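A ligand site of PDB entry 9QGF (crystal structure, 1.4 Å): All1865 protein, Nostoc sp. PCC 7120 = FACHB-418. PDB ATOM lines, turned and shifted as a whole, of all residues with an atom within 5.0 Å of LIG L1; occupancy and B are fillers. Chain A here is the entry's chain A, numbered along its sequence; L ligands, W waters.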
ATOM      1  N   ALA A  35     -31.320  20.807 -12.050  1.00  0.00           N
ATOM      2  CA  ALA A  35     -30.569  19.557 -12.020  1.00  0.00           C
ATOM      3  C   ALA A  35     -29.444  19.668 -10.994  1.00  0.00           C
ATOM      4  O   ALA A  35     -28.945  20.779 -10.684  1.00  0.00           O
ATOM      5  CB  ALA A  35     -30.026  19.255 -13.422  1.00  0.00           C
ATOM      6  N   PRO A  36     -28.990  18.505 -10.448  1.00  0.00           N
ATOM      7  CA  PRO A  36     -27.826  18.498  -9.545  1.00  0.00           C
ATOM      8  C   PRO A  36     -26.547  18.916 -10.246  1.00  0.00           C
ATOM      9  O   PRO A  36     -26.245  18.422 -11.335  1.00  0.00           O
ATOM     10  CB  PRO A  36     -27.695  17.032  -9.098  1.00  0.00           C
ATOM     11  CG  PRO A  36     -28.455  16.230 -10.168  1.00  0.00           C
ATOM     12  CD  PRO A  36     -29.557  17.162 -10.702  1.00  0.00           C
ATOM     13  N   LEU A  37     -25.821  19.862  -9.614  1.00  0.00           N
ATOM     14  CA  LEU A  37     -24.624  20.399 -10.262  1.00  0.00           C
ATOM     15  C   LEU A  37     -23.492  20.527  -9.253  1.00  0.00           C
ATOM     16  O   LEU A  37     -23.556  21.359  -8.333  1.00  0.00           O
ATOM     17  CB  LEU A  37     -24.874  21.778 -10.871  1.00  0.00           C
ATOM     18  CG  LEU A  37     -25.973  21.829 -11.942  1.00  0.00           C
ATOM     19  CD1 LEU A  37     -26.595  23.243 -12.021  1.00  0.00           C
ATOM     20  CD2 LEU A  37     -25.388  21.440 -13.317  1.00  0.00           C
ATOM     21  N   THR A  38     -22.479  19.687  -9.435  1.00  0.00           N
ATOM     22  CA  THR A  38     -21.289  19.793  -8.597  1.00  0.00           C
ATOM     23  C   THR A  38     -20.591  21.115  -8.860  1.00  0.00           C
ATOM     24  O   THR A  38     -20.285  21.440 -10.016  1.00  0.00           O
ATOM     25  CB  THR A  38     -20.336  18.659  -8.982  1.00  0.00           C
ATOM     26  OG1 THR A  38     -20.908  17.440  -8.514  1.00  0.00           O
ATOM     27  CG2 THR A  38     -18.934  18.852  -8.400  1.00  0.00           C
ATOM     28  N   ARG A  39     -20.355  21.883  -7.792  1.00  0.00           N
ATOM     29  CA  ARG A  39     -19.716  23.208  -7.935  1.00  0.00           C
ATOM     30  C   ARG A  39     -18.414  23.274  -7.130  1.00  0.00           C
ATOM     31  O   ARG A  39     -17.670  24.267  -7.251  1.00  0.00           O
ATOM     32  CB  ARG A  39     -20.651  24.378  -7.536  1.00  0.00           C
ATOM     33  CG  ARG A  39     -22.032  24.324  -8.200  1.00  0.00           C
ATOM     34  CD  ARG A  39     -21.953  24.282  -9.774  1.00  0.00           C
ATOM     35  NE  ARG A  39     -21.167  25.414 -10.300  1.00  0.00           N
ATOM     36  CZ  ARG A  39     -21.639  26.669 -10.403  1.00  0.00           C
ATOM     37  NH1 ARG A  39     -22.932  26.944 -10.154  1.00  0.00           N
ATOM     38  NH2 ARG A  39     -20.808  27.627 -10.825  1.00  0.00           N
ATOM     39  N   GLU A  68     -26.446  19.631  -5.490  1.00  0.00           N
ATOM     40  CA  GLU A  68     -25.253  18.965  -6.005  1.00  0.00           C
ATOM     41  C   GLU A  68     -25.058  17.590  -5.348  1.00  0.00           C
ATOM     42  O   GLU A  68     -25.381  17.405  -4.164  1.00  0.00           O
ATOM     43  CB  GLU A  68     -24.040  19.859  -5.706  1.00  0.00           C
ATOM     44  CG  GLU A  68     -23.768  20.033  -4.216  1.00  0.00           C
ATOM     45  CD  GLU A  68     -23.042  21.323  -3.943  1.00  0.00           C
ATOM     46  OE1 GLU A  68     -21.795  21.396  -4.091  1.00  0.00           O
ATOM     47  OE2 GLU A  68     -23.762  22.279  -3.625  1.00  0.00           O
ATOM     48  N   ALA A  69     -24.374  16.708  -6.084  1.00  0.00           N
ATOM     49  CA  ALA A  69     -23.962  15.415  -5.527  1.00  0.00           C
ATOM     50  C   ALA A  69     -23.183  15.615  -4.229  1.00  0.00           C
ATOM     51  O   ALA A  69     -22.252  16.426  -4.160  1.00  0.00           O
ATOM     52  CB  ALA A  69     -23.168  14.649  -6.575  1.00  0.00           C
ATOM     53  N   GLN A 111     -28.922  15.394  -3.466  1.00  0.00           N
ATOM     54  CA  GLN A 111     -28.466  14.243  -4.224  1.00  0.00           C
ATOM     55  C   GLN A 111     -27.399  13.504  -3.421  1.00  0.00           C
ATOM     56  O   GLN A 111     -26.358  14.085  -3.082  1.00  0.00           O
ATOM     57  CB  GLN A 111     -27.950  14.642  -5.602  1.00  0.00           C
ATOM     58  CG  GLN A 111     -27.787  13.405  -6.497  1.00  0.00           C
ATOM     59  CD  GLN A 111     -27.067  13.658  -7.792  1.00  0.00           C
ATOM     60  OE1 GLN A 111     -25.980  14.255  -7.833  1.00  0.00           O
ATOM     61  NE2 GLN A 111     -27.655  13.179  -8.893  1.00  0.00           N
ATOM     62  N   HIS A 187     -28.090   9.074  -6.392  1.00  0.00           N
ATOM     63  CA  HIS A 187     -27.332   9.227  -7.627  1.00  0.00           C
ATOM     64  C   HIS A 187     -26.900   7.855  -8.100  1.00  0.00           C
ATOM     65  O   HIS A 187     -25.926   7.271  -7.604  1.00  0.00           O
ATOM     66  CB  HIS A 187     -26.074  10.067  -7.345  1.00  0.00           C
ATOM     67  CG  HIS A 187     -25.381  10.598  -8.559  1.00  0.00           C
ATOM     68  ND1 HIS A 187     -25.579  10.044  -9.806  1.00  0.00           N
ATOM     69  CD2 HIS A 187     -24.432  11.543  -8.678  1.00  0.00           C
ATOM     70  CE1 HIS A 187     -24.785  10.683 -10.678  1.00  0.00           C
ATOM     71  NE2 HIS A 187     -24.101  11.656 -10.012  1.00  0.00           N
ATOM     72  N   ASN A 190     -24.016   8.507 -14.074  1.00  0.00           N
ATOM     73  CA  ASN A 190     -22.715   9.075 -14.384  1.00  0.00           C
ATOM     74  C   ASN A 190     -21.518   8.206 -14.027  1.00  0.00           C
ATOM     75  O   ASN A 190     -20.407   8.747 -13.911  1.00  0.00           O
ATOM     76  CB  ASN A 190     -22.609  10.524 -13.903  1.00  0.00           C
ATOM     77  CG  ASN A 190     -23.709  11.358 -14.550  1.00  0.00           C
ATOM     78  OD1 ASN A 190     -24.246  10.979 -15.623  1.00  0.00           O
ATOM     79  ND2 ASN A 190     -24.041  12.483 -13.940  1.00  0.00           N
ATOM     80  N   ARG A 239     -31.797   8.771  -9.858  1.00  0.00           N
ATOM     81  CA  ARG A 239     -31.342   9.289 -11.163  1.00  0.00           C
ATOM     82  C   ARG A 239     -30.514   8.231 -11.875  1.00  0.00           C
ATOM     83  O   ARG A 239     -29.639   7.621 -11.267  1.00  0.00           O
ATOM     84  CB  ARG A 239     -30.444  10.528 -10.934  1.00  0.00           C
ATOM     85  CG  ARG A 239     -30.202  11.273 -12.252  1.00  0.00           C
ATOM     86  CD  ARG A 239     -29.447  12.611 -12.080  1.00  0.00           C
ATOM     87  NE  ARG A 239     -29.841  13.489 -13.193  1.00  0.00           N
ATOM     88  CZ  ARG A 239     -29.146  14.523 -13.668  1.00  0.00           C
ATOM     89  NH1 ARG A 239     -27.866  14.726 -13.344  1.00  0.00           N
ATOM     90  NH2 ARG A 239     -29.768  15.388 -14.460  1.00  0.00           N
ATOM     91  N   PHE A 276     -31.067  11.472 -17.040  1.00  0.00           N
ATOM     92  CA  PHE A 276     -30.141  12.337 -17.752  1.00  0.00           C
ATOM     93  C   PHE A 276     -29.938  11.668 -19.115  1.00  0.00           C
ATOM     94  O   PHE A 276     -29.361  10.574 -19.188  1.00  0.00           O
ATOM     95  CB  PHE A 276     -28.855  12.437 -16.921  1.00  0.00           C
ATOM     96  CG  PHE A 276     -27.666  13.094 -17.610  1.00  0.00           C
ATOM     97  CD1 PHE A 276     -27.775  13.883 -18.772  1.00  0.00           C
ATOM     98  CD2 PHE A 276     -26.396  12.815 -17.119  1.00  0.00           C
ATOM     99  CE1 PHE A 276     -26.644  14.424 -19.383  1.00  0.00           C
ATOM    100  CE2 PHE A 276     -25.271  13.390 -17.723  1.00  0.00           C
ATOM    101  CZ  PHE A 276     -25.393  14.177 -18.852  1.00  0.00           C
ATOM    102  N   ILE A 279     -26.145  13.905 -24.224  1.00  0.00           N
ATOM    103  CA  ILE A 279     -26.279  14.778 -25.380  1.00  0.00           C
ATOM    104  C   ILE A 279     -25.584  14.152 -26.597  1.00  0.00           C
ATOM    105  O   ILE A 279     -25.897  14.559 -27.728  1.00  0.00           O
ATOM    106  CB  ILE A 279     -25.671  16.160 -25.046  1.00  0.00           C
ATOM    107  CG1 ILE A 279     -26.423  16.830 -23.892  1.00  0.00           C
ATOM    108  CG2 ILE A 279     -25.585  17.089 -26.255  1.00  0.00           C
ATOM    109  CD1 ILE A 279     -27.932  16.799 -24.021  1.00  0.00           C
ATOM    110  N   ASN A 306     -33.954  15.270 -18.745  1.00  0.00           N
ATOM    111  CA  ASN A 306     -32.886  16.252 -18.633  1.00  0.00           C
ATOM    112  C   ASN A 306     -31.896  16.029 -19.773  1.00  0.00           C
ATOM    113  O   ASN A 306     -31.727  14.905 -20.229  1.00  0.00           O
ATOM    114  CB  ASN A 306     -32.160  16.097 -17.305  1.00  0.00           C
ATOM    115  CG  ASN A 306     -30.789  16.742 -17.362  1.00  0.00           C
ATOM    116  OD1 ASN A 306     -29.800  16.045 -17.658  1.00  0.00           O
ATOM    117  ND2 ASN A 306     -30.690  18.056 -17.147  1.00  0.00           N
ATOM    118  N   GLY A 307     -31.313  17.141 -20.264  1.00  0.00           N
ATOM    119  CA  GLY A 307     -30.243  17.054 -21.233  1.00  0.00           C
ATOM    120  C   GLY A 307     -30.558  17.940 -22.437  1.00  0.00           C
ATOM    121  O   GLY A 307     -31.289  17.549 -23.321  1.00  0.00           O
ATOM    122  N   GLY A 308     -30.016  19.160 -22.412  1.00  0.00           N
ATOM    123  CA  GLY A 308     -30.108  20.103 -23.519  1.00  0.00           C
ATOM    124  C   GLY A 308     -31.527  20.640 -23.724  1.00  0.00           C
ATOM    125  O   GLY A 308     -31.877  21.041 -24.828  1.00  0.00           O
ATOM    126  N   TYR A 309     -32.348  20.684 -22.667  1.00  0.00           N
ATOM    127  CA  TYR A 309     -33.696  21.230 -22.793  1.00  0.00           C
ATOM    128  C   TYR A 309     -33.730  22.760 -22.925  1.00  0.00           C
ATOM    129  O   TYR A 309     -32.803  23.487 -22.549  1.00  0.00           O
ATOM    130  CB  TYR A 309     -34.669  20.723 -21.717  1.00  0.00           C
ATOM    131  CG  TYR A 309     -35.094  19.291 -22.025  1.00  0.00           C
ATOM    132  CD1 TYR A 309     -34.303  18.217 -21.630  1.00  0.00           C
ATOM    133  CD2 TYR A 309     -36.252  19.019 -22.746  1.00  0.00           C
ATOM    134  CE1 TYR A 309     -34.626  16.913 -21.950  1.00  0.00           C
ATOM    135  CE2 TYR A 309     -36.595  17.716 -23.056  1.00  0.00           C
ATOM    136  CZ  TYR A 309     -35.780  16.664 -22.664  1.00  0.00           C
ATOM    137  OH  TYR A 309     -36.106  15.367 -22.961  1.00  0.00           O
ATOM    138  N   ALA A 327     -35.599  18.910 -15.987  1.00  0.00           N
ATOM    139  CA  ALA A 327     -34.495  19.513 -15.238  1.00  0.00           C
ATOM    140  C   ALA A 327     -33.505  20.155 -16.189  1.00  0.00           C
ATOM    141  O   ALA A 327     -33.203  19.620 -17.257  1.00  0.00           O
ATOM    142  CB  ALA A 327     -33.825  18.469 -14.336  1.00  0.00           C
ATOM    143  N   PHE A 328     -33.006  21.343 -15.756  1.00  0.00           N
ATOM    144  CA  PHE A 328     -32.018  22.119 -16.481  1.00  0.00           C
ATOM    145  C   PHE A 328     -30.778  22.245 -15.603  1.00  0.00           C
ATOM    146  O   PHE A 328     -30.891  22.616 -14.415  1.00  0.00           O
ATOM    147  CB  PHE A 328     -32.568  23.544 -16.705  1.00  0.00           C
ATOM    148  CG  PHE A 328     -33.802  23.572 -17.598  1.00  0.00           C
ATOM    149  CD1 PHE A 328     -35.075  23.346 -17.081  1.00  0.00           C
ATOM    150  CD2 PHE A 328     -33.675  23.892 -18.955  1.00  0.00           C
ATOM    151  CE1 PHE A 328     -36.196  23.366 -17.918  1.00  0.00           C
ATOM    152  CE2 PHE A 328     -34.798  23.939 -19.779  1.00  0.00           C
ATOM    153  CZ  PHE A 328     -36.042  23.682 -19.262  1.00  0.00           C
ATOM    154  N   GLY A 329     -29.602  21.906 -16.158  1.00  0.00           N
ATOM    155  CA  GLY A 329     -28.347  22.016 -15.436  1.00  0.00           C
ATOM    156  C   GLY A 329     -27.647  23.310 -15.833  1.00  0.00           C
ATOM    157  O   GLY A 329     -27.726  24.315 -15.107  1.00  0.00           O
ATOM    158  N   THR A 330     -27.015  23.262 -17.012  1.00  0.00           N
ATOM    159  CA  THR A 330     -26.222  24.391 -17.484  1.00  0.00           C
ATOM    160  C   THR A 330     -26.967  25.736 -17.349  1.00  0.00           C
ATOM    161  O   THR A 330     -26.395  26.710 -16.852  1.00  0.00           O
ATOM    162  CB  THR A 330     -25.708  24.180 -18.917  1.00  0.00           C
ATOM    163  OG1 THR A 330     -25.094  22.886 -18.909  1.00  0.00           O
ATOM    164  CG2 THR A 330     -24.675  25.246 -19.272  1.00  0.00           C
ATOM    165  N   ILE A 333     -26.980  27.245 -13.941  1.00  0.00           N
ATOM    166  CA  ILE A 333     -25.729  27.823 -13.483  1.00  0.00           C
ATOM    167  C   ILE A 333     -25.797  29.329 -13.741  1.00  0.00           C
ATOM    168  O   ILE A 333     -25.528  30.149 -12.847  1.00  0.00           O
ATOM    169  CB  ILE A 333     -24.496  27.185 -14.169  1.00  0.00           C
ATOM    170  CG1 ILE A 333     -24.392  25.703 -13.754  1.00  0.00           C
ATOM    171  CG2 ILE A 333     -23.222  27.952 -13.833  1.00  0.00           C
ATOM    172  CD1 ILE A 333     -23.225  24.904 -14.345  1.00  0.00           C
ATOM    173  N   PHE A 356     -17.234  26.832 -13.410  1.00  0.00           N
ATOM    174  CA  PHE A 356     -18.149  25.802 -12.944  1.00  0.00           C
ATOM    175  C   PHE A 356     -17.640  25.133 -11.662  1.00  0.00           C
ATOM    176  O   PHE A 356     -18.431  24.958 -10.717  1.00  0.00           O
ATOM    177  CB  PHE A 356     -18.338  24.657 -13.963  1.00  0.00           C
ATOM    178  CG  PHE A 356     -19.139  25.044 -15.202  1.00  0.00           C
ATOM    179  CD1 PHE A 356     -19.767  26.295 -15.277  1.00  0.00           C
ATOM    180  CD2 PHE A 356     -19.361  24.103 -16.226  1.00  0.00           C
ATOM    181  CE1 PHE A 356     -20.501  26.629 -16.393  1.00  0.00           C
ATOM    182  CE2 PHE A 356     -20.108  24.453 -17.349  1.00  0.00           C
ATOM    183  CZ  PHE A 356     -20.677  25.703 -17.424  1.00  0.00           C
ATOM    184  N   TYR A 357     -16.349  24.757 -11.637  1.00  0.00           N
ATOM    185  CA  TYR A 357     -15.863  23.978 -10.485  1.00  0.00           C
ATOM    186  C   TYR A 357     -14.822  24.726  -9.651  1.00  0.00           C
ATOM    187  O   TYR A 357     -13.825  25.217 -10.187  1.00  0.00           O
ATOM    188  CB  TYR A 357     -15.197  22.714 -11.024  1.00  0.00           C
ATOM    189  CG  TYR A 357     -16.090  21.833 -11.869  1.00  0.00           C
ATOM    190  CD1 TYR A 357     -17.122  21.113 -11.291  1.00  0.00           C
ATOM    191  CD2 TYR A 357     -15.887  21.735 -13.247  1.00  0.00           C
ATOM    192  CE1 TYR A 357     -17.900  20.254 -12.050  1.00  0.00           C
ATOM    193  CE2 TYR A 357     -16.686  20.896 -14.007  1.00  0.00           C
ATOM    194  CZ  TYR A 357     -17.697  20.175 -13.408  1.00  0.00           C
ATOM    195  OH  TYR A 357     -18.462  19.349 -14.172  1.00  0.00           O
HETATM  196  N1  LIG L   1     -25.154  15.358 -12.607  1.00  0.00           N
HETATM  197  C1  LIG L   1     -25.382  14.755 -11.423  1.00  0.00           C
HETATM  198  O1  LIG L   1     -26.162  13.786 -11.365  1.00  0.00           O
HETATM  199  N2  LIG L   1     -24.820  15.188 -10.235  1.00  0.00           N
HETATM  200  C2  LIG L   1     -23.915  16.219 -10.218  1.00  0.00           C
HETATM  201  O2  LIG L   1     -23.508  16.641  -9.145  1.00  0.00           O
HETATM  202  C3  LIG L   1     -23.647  16.881 -11.452  1.00  0.00           C
HETATM  203  N3  LIG L   1     -22.716  17.867 -11.492  1.00  0.00           N
HETATM  204  C4  LIG L   1     -22.588  18.542 -12.675  1.00  0.00           C
HETATM  205  C5  LIG L   1     -21.757  19.667 -12.692  1.00  0.00           C
HETATM  206  C6  LIG L   1     -21.682  20.497 -13.799  1.00  0.00           C
HETATM  207  C7  LIG L   1     -20.806  21.735 -13.770  1.00  0.00           C
HETATM  208  C8  LIG L   1     -22.359  20.129 -15.000  1.00  0.00           C
HETATM  209  C9  LIG L   1     -22.275  20.987 -16.248  1.00  0.00           C
HETATM  210  C10 LIG L   1     -23.074  18.938 -15.031  1.00  0.00           C
HETATM  211  C11 LIG L   1     -23.235  18.164 -13.857  1.00  0.00           C
HETATM  212  N4  LIG L   1     -24.058  17.035 -13.817  1.00  0.00           N
HETATM  213  C12 LIG L   1     -24.332  16.396 -12.616  1.00  0.00           C
HETATM  214  C13 LIG L   1     -24.927  16.708 -14.943  1.00  0.00           C
HETATM  215  C14 LIG L   1     -26.116  17.713 -14.944  1.00  0.00           C
HETATM  216  O3  LIG L   1     -26.987  17.491 -13.828  1.00  0.00           O
HETATM  217  C15 LIG L   1     -26.989  17.598 -16.186  1.00  0.00           C
HETATM  218  O4  LIG L   1     -27.553  16.287 -16.230  1.00  0.00           O
HETATM  219  C16 LIG L   1     -26.239  17.840 -17.491  1.00  0.00           C
HETATM  220  O5  LIG L   1     -25.460  19.034 -17.384  1.00  0.00           O
HETATM  221  C17 LIG L   1     -27.152  17.893 -18.710  1.00  0.00           C
HETATM  222  O6  LIG L   1     -28.224  18.854 -18.528  1.00  0.00           O
HETATM  223  P1  LIG L   1     -28.136  20.334 -19.188  1.00  0.00           P
HETATM  224  O7  LIG L   1     -29.465  21.008 -18.808  1.00  0.00           O
HETATM  225  O8  LIG L   1     -28.020  20.133 -20.701  1.00  0.00           O
HETATM  226  O9  LIG L   1     -26.916  20.991 -18.577  1.00  0.00           O
HETATM  227  C1  LG2 L   2     -21.351  13.917  -9.702  1.00  0.00           C
HETATM  228  C2  LG2 L   2     -21.560  14.108 -11.171  1.00  0.00           C
HETATM  229  O1  LG2 L   2     -22.435  13.500 -11.619  1.00  0.00           O
HETATM  230  C3  LG2 L   2     -20.771  14.920 -12.138  1.00  0.00           C
HETATM  231  C4  LG2 L   2     -21.235  14.846 -13.614  1.00  0.00           C
HETATM  232  C5  LG2 L   2     -20.191  15.195 -14.643  1.00  0.00           C
HETATM  233  C6  LG2 L   2     -20.726  15.260 -16.095  1.00  0.00           C
HETATM  234  C7  LG2 L   2     -22.186  15.207 -16.375  1.00  0.00           C
HETATM  235  O2  LG2 L   2     -19.956  15.305 -17.039  1.00  0.00           O
HETATM  236  C8  LG2 L   2     -19.165  14.013 -14.679  1.00  0.00           C
HETATM  237  C9  LG2 L   2     -19.818  12.676 -14.512  1.00  0.00           C
HETATM  238  O3  LG2 L   2     -17.952  14.054 -14.813  1.00  0.00           O
HETATM  239  C10 LG2 L   2     -19.487  16.533 -14.266  1.00  0.00           C
HETATM  240  C11 LG2 L   2     -19.164  16.726 -12.797  1.00  0.00           C
HETATM  241  C12 LG2 L   2     -19.545  15.630 -11.865  1.00  0.00           C
HETATM  242  C13 LG2 L   2     -19.025  15.533 -10.469  1.00  0.00           C
HETATM  243  O   HOH W   1     -31.785  19.928 -19.706  1.00  0.00           O
HETATM  244  O   HOH W   2     -21.026  19.530 -19.148  1.00  0.00           O
HETATM  245  O   HOH W   3     -25.586  19.553 -21.871  1.00  0.00           O
HETATM  246  O   HOH W   4     -27.844  22.337 -22.250  1.00  0.00           O
HETATM  247  O   HOH W   5     -23.218  18.172 -18.877  1.00  0.00           O
HETATM  248  O   HOH W   6     -29.716  23.703 -19.152  1.00  0.00           O
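The backbone NH (N) of Thr 330 sits at hydrogen-bond distance from an oxygen (O9) of LIG L1.
An oxygen (O9) of LIG L1 sits at hydrogen-bond distance from the side-chain hydroxyl (OG1) of Thr 330, 2.6 Å away.
OD1 of Asn 306 is in hydrogen-bond range of O4 of LIG L1 (2.7 Å).
The backbone NH (N) of Thr 38 lies within hydrogen-bond range of a nitrogen (N3) of LIG L1.
OG1 of Thr 38 lies within hydrogen-bond range of O2 of LIG L1, at 2.8 Å.
O of Pro 36 lies within hydrogen-bond range of O3 of LIG L1 (2.8 Å).
The guanidinium group (NH1) of Arg 239 lies within hydrogen-bond range of an oxygen (O1) of LIG L1 (2.8 Å).
The backbone NH of Gly 329 lies within hydrogen-bond range of an oxygen (O7) of LIG L1 (2.8 Å).
An oxygen (O8) of LIG L1 sits at hydrogen-bond distance from the backbone NH (N) of Gly 308 (2.8 Å).
The side-chain amide oxygen (OE1) of Gln 111 lies within hydrogen-bond range of a nitrogen (N2) of LIG L1 (2.8 Å).
O2 of LIG L1 lies within hydrogen-bond range of N of Ala 69 (3.2 Å).
A ring nitrogen (NE2) of His 187 lies within hydrogen-bond range of an oxygen (O1) of LIG L1 (3.3 Å).
N1 of LIG L1 lies within hydrogen-bond range of ND2 of Asn 190 (3.4 Å).
NE2 of His 187 is in hydrogen-bond range of O1 of LG2 L2.
An oxygen (O1) of LG2 L2 lies within hydrogen-bond range of the side-chain amide nitrogen (ND2) of Asn 190, at 3.0 Å.
N2 of LIG L1 sits close to O1 of LG2 L2, at 3.2 Å.
The side-chain amide oxygen (OD1) of Asn 306 is in hydrogen-bond range of the guanidinium group (NH2) of Arg 239 (3.3 Å).
The side-chain amide nitrogen of Asn 306 lies within hydrogen-bond range of the backbone carbonyl oxygen of Ala 327 (3.0 Å).
The side-chain amide oxygen of Gln 111 lies close to the backbone NH of Ala 69 (3.4 Å).
The backbone NH (N) of Ala 35 sits at hydrogen-bond distance from the backbone carbonyl oxygen (O) of Phe 328, at 3.0 Å.
NE of Arg 39 sits at hydrogen-bond distance from O of Phe 356, 2.8 Å away.
Residues that only touch LIG L1: Ala 35 (3.5 Å), Leu 37 (3.4 Å), Phe 276 (3.5 Å), Gly 307 (3.8 Å), Phe 328 (3.6 Å), Phe 356 (3.7 Å) and Tyr 357 (3.4 Å).
Hydrophobic or aromatic side chains that line LIG L1: Ala 35, Pro 36, Leu 37, Ala 69, His 187, Phe 276, Phe 356 and Tyr 357.
18 residues have an atom within 4 Å of LIG L1: Ala 35, Pro 36, Leu 37, Thr 38, Ala 69, Gln 111, His 187, Asn 190, Arg 239, Phe 276, Asn 306, Gly 307, Gly 308, Phe 328, Gly 329, Thr 330, Phe 356 and Tyr 357.
Water W6 lies within hydrogen-bond range of an oxygen (O7) of LIG L1 (2.7 Å), the backbone NH (N) of Thr 330 (3.5 Å) and the backbone NH (N) of Gly 329 (3.5 Å).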
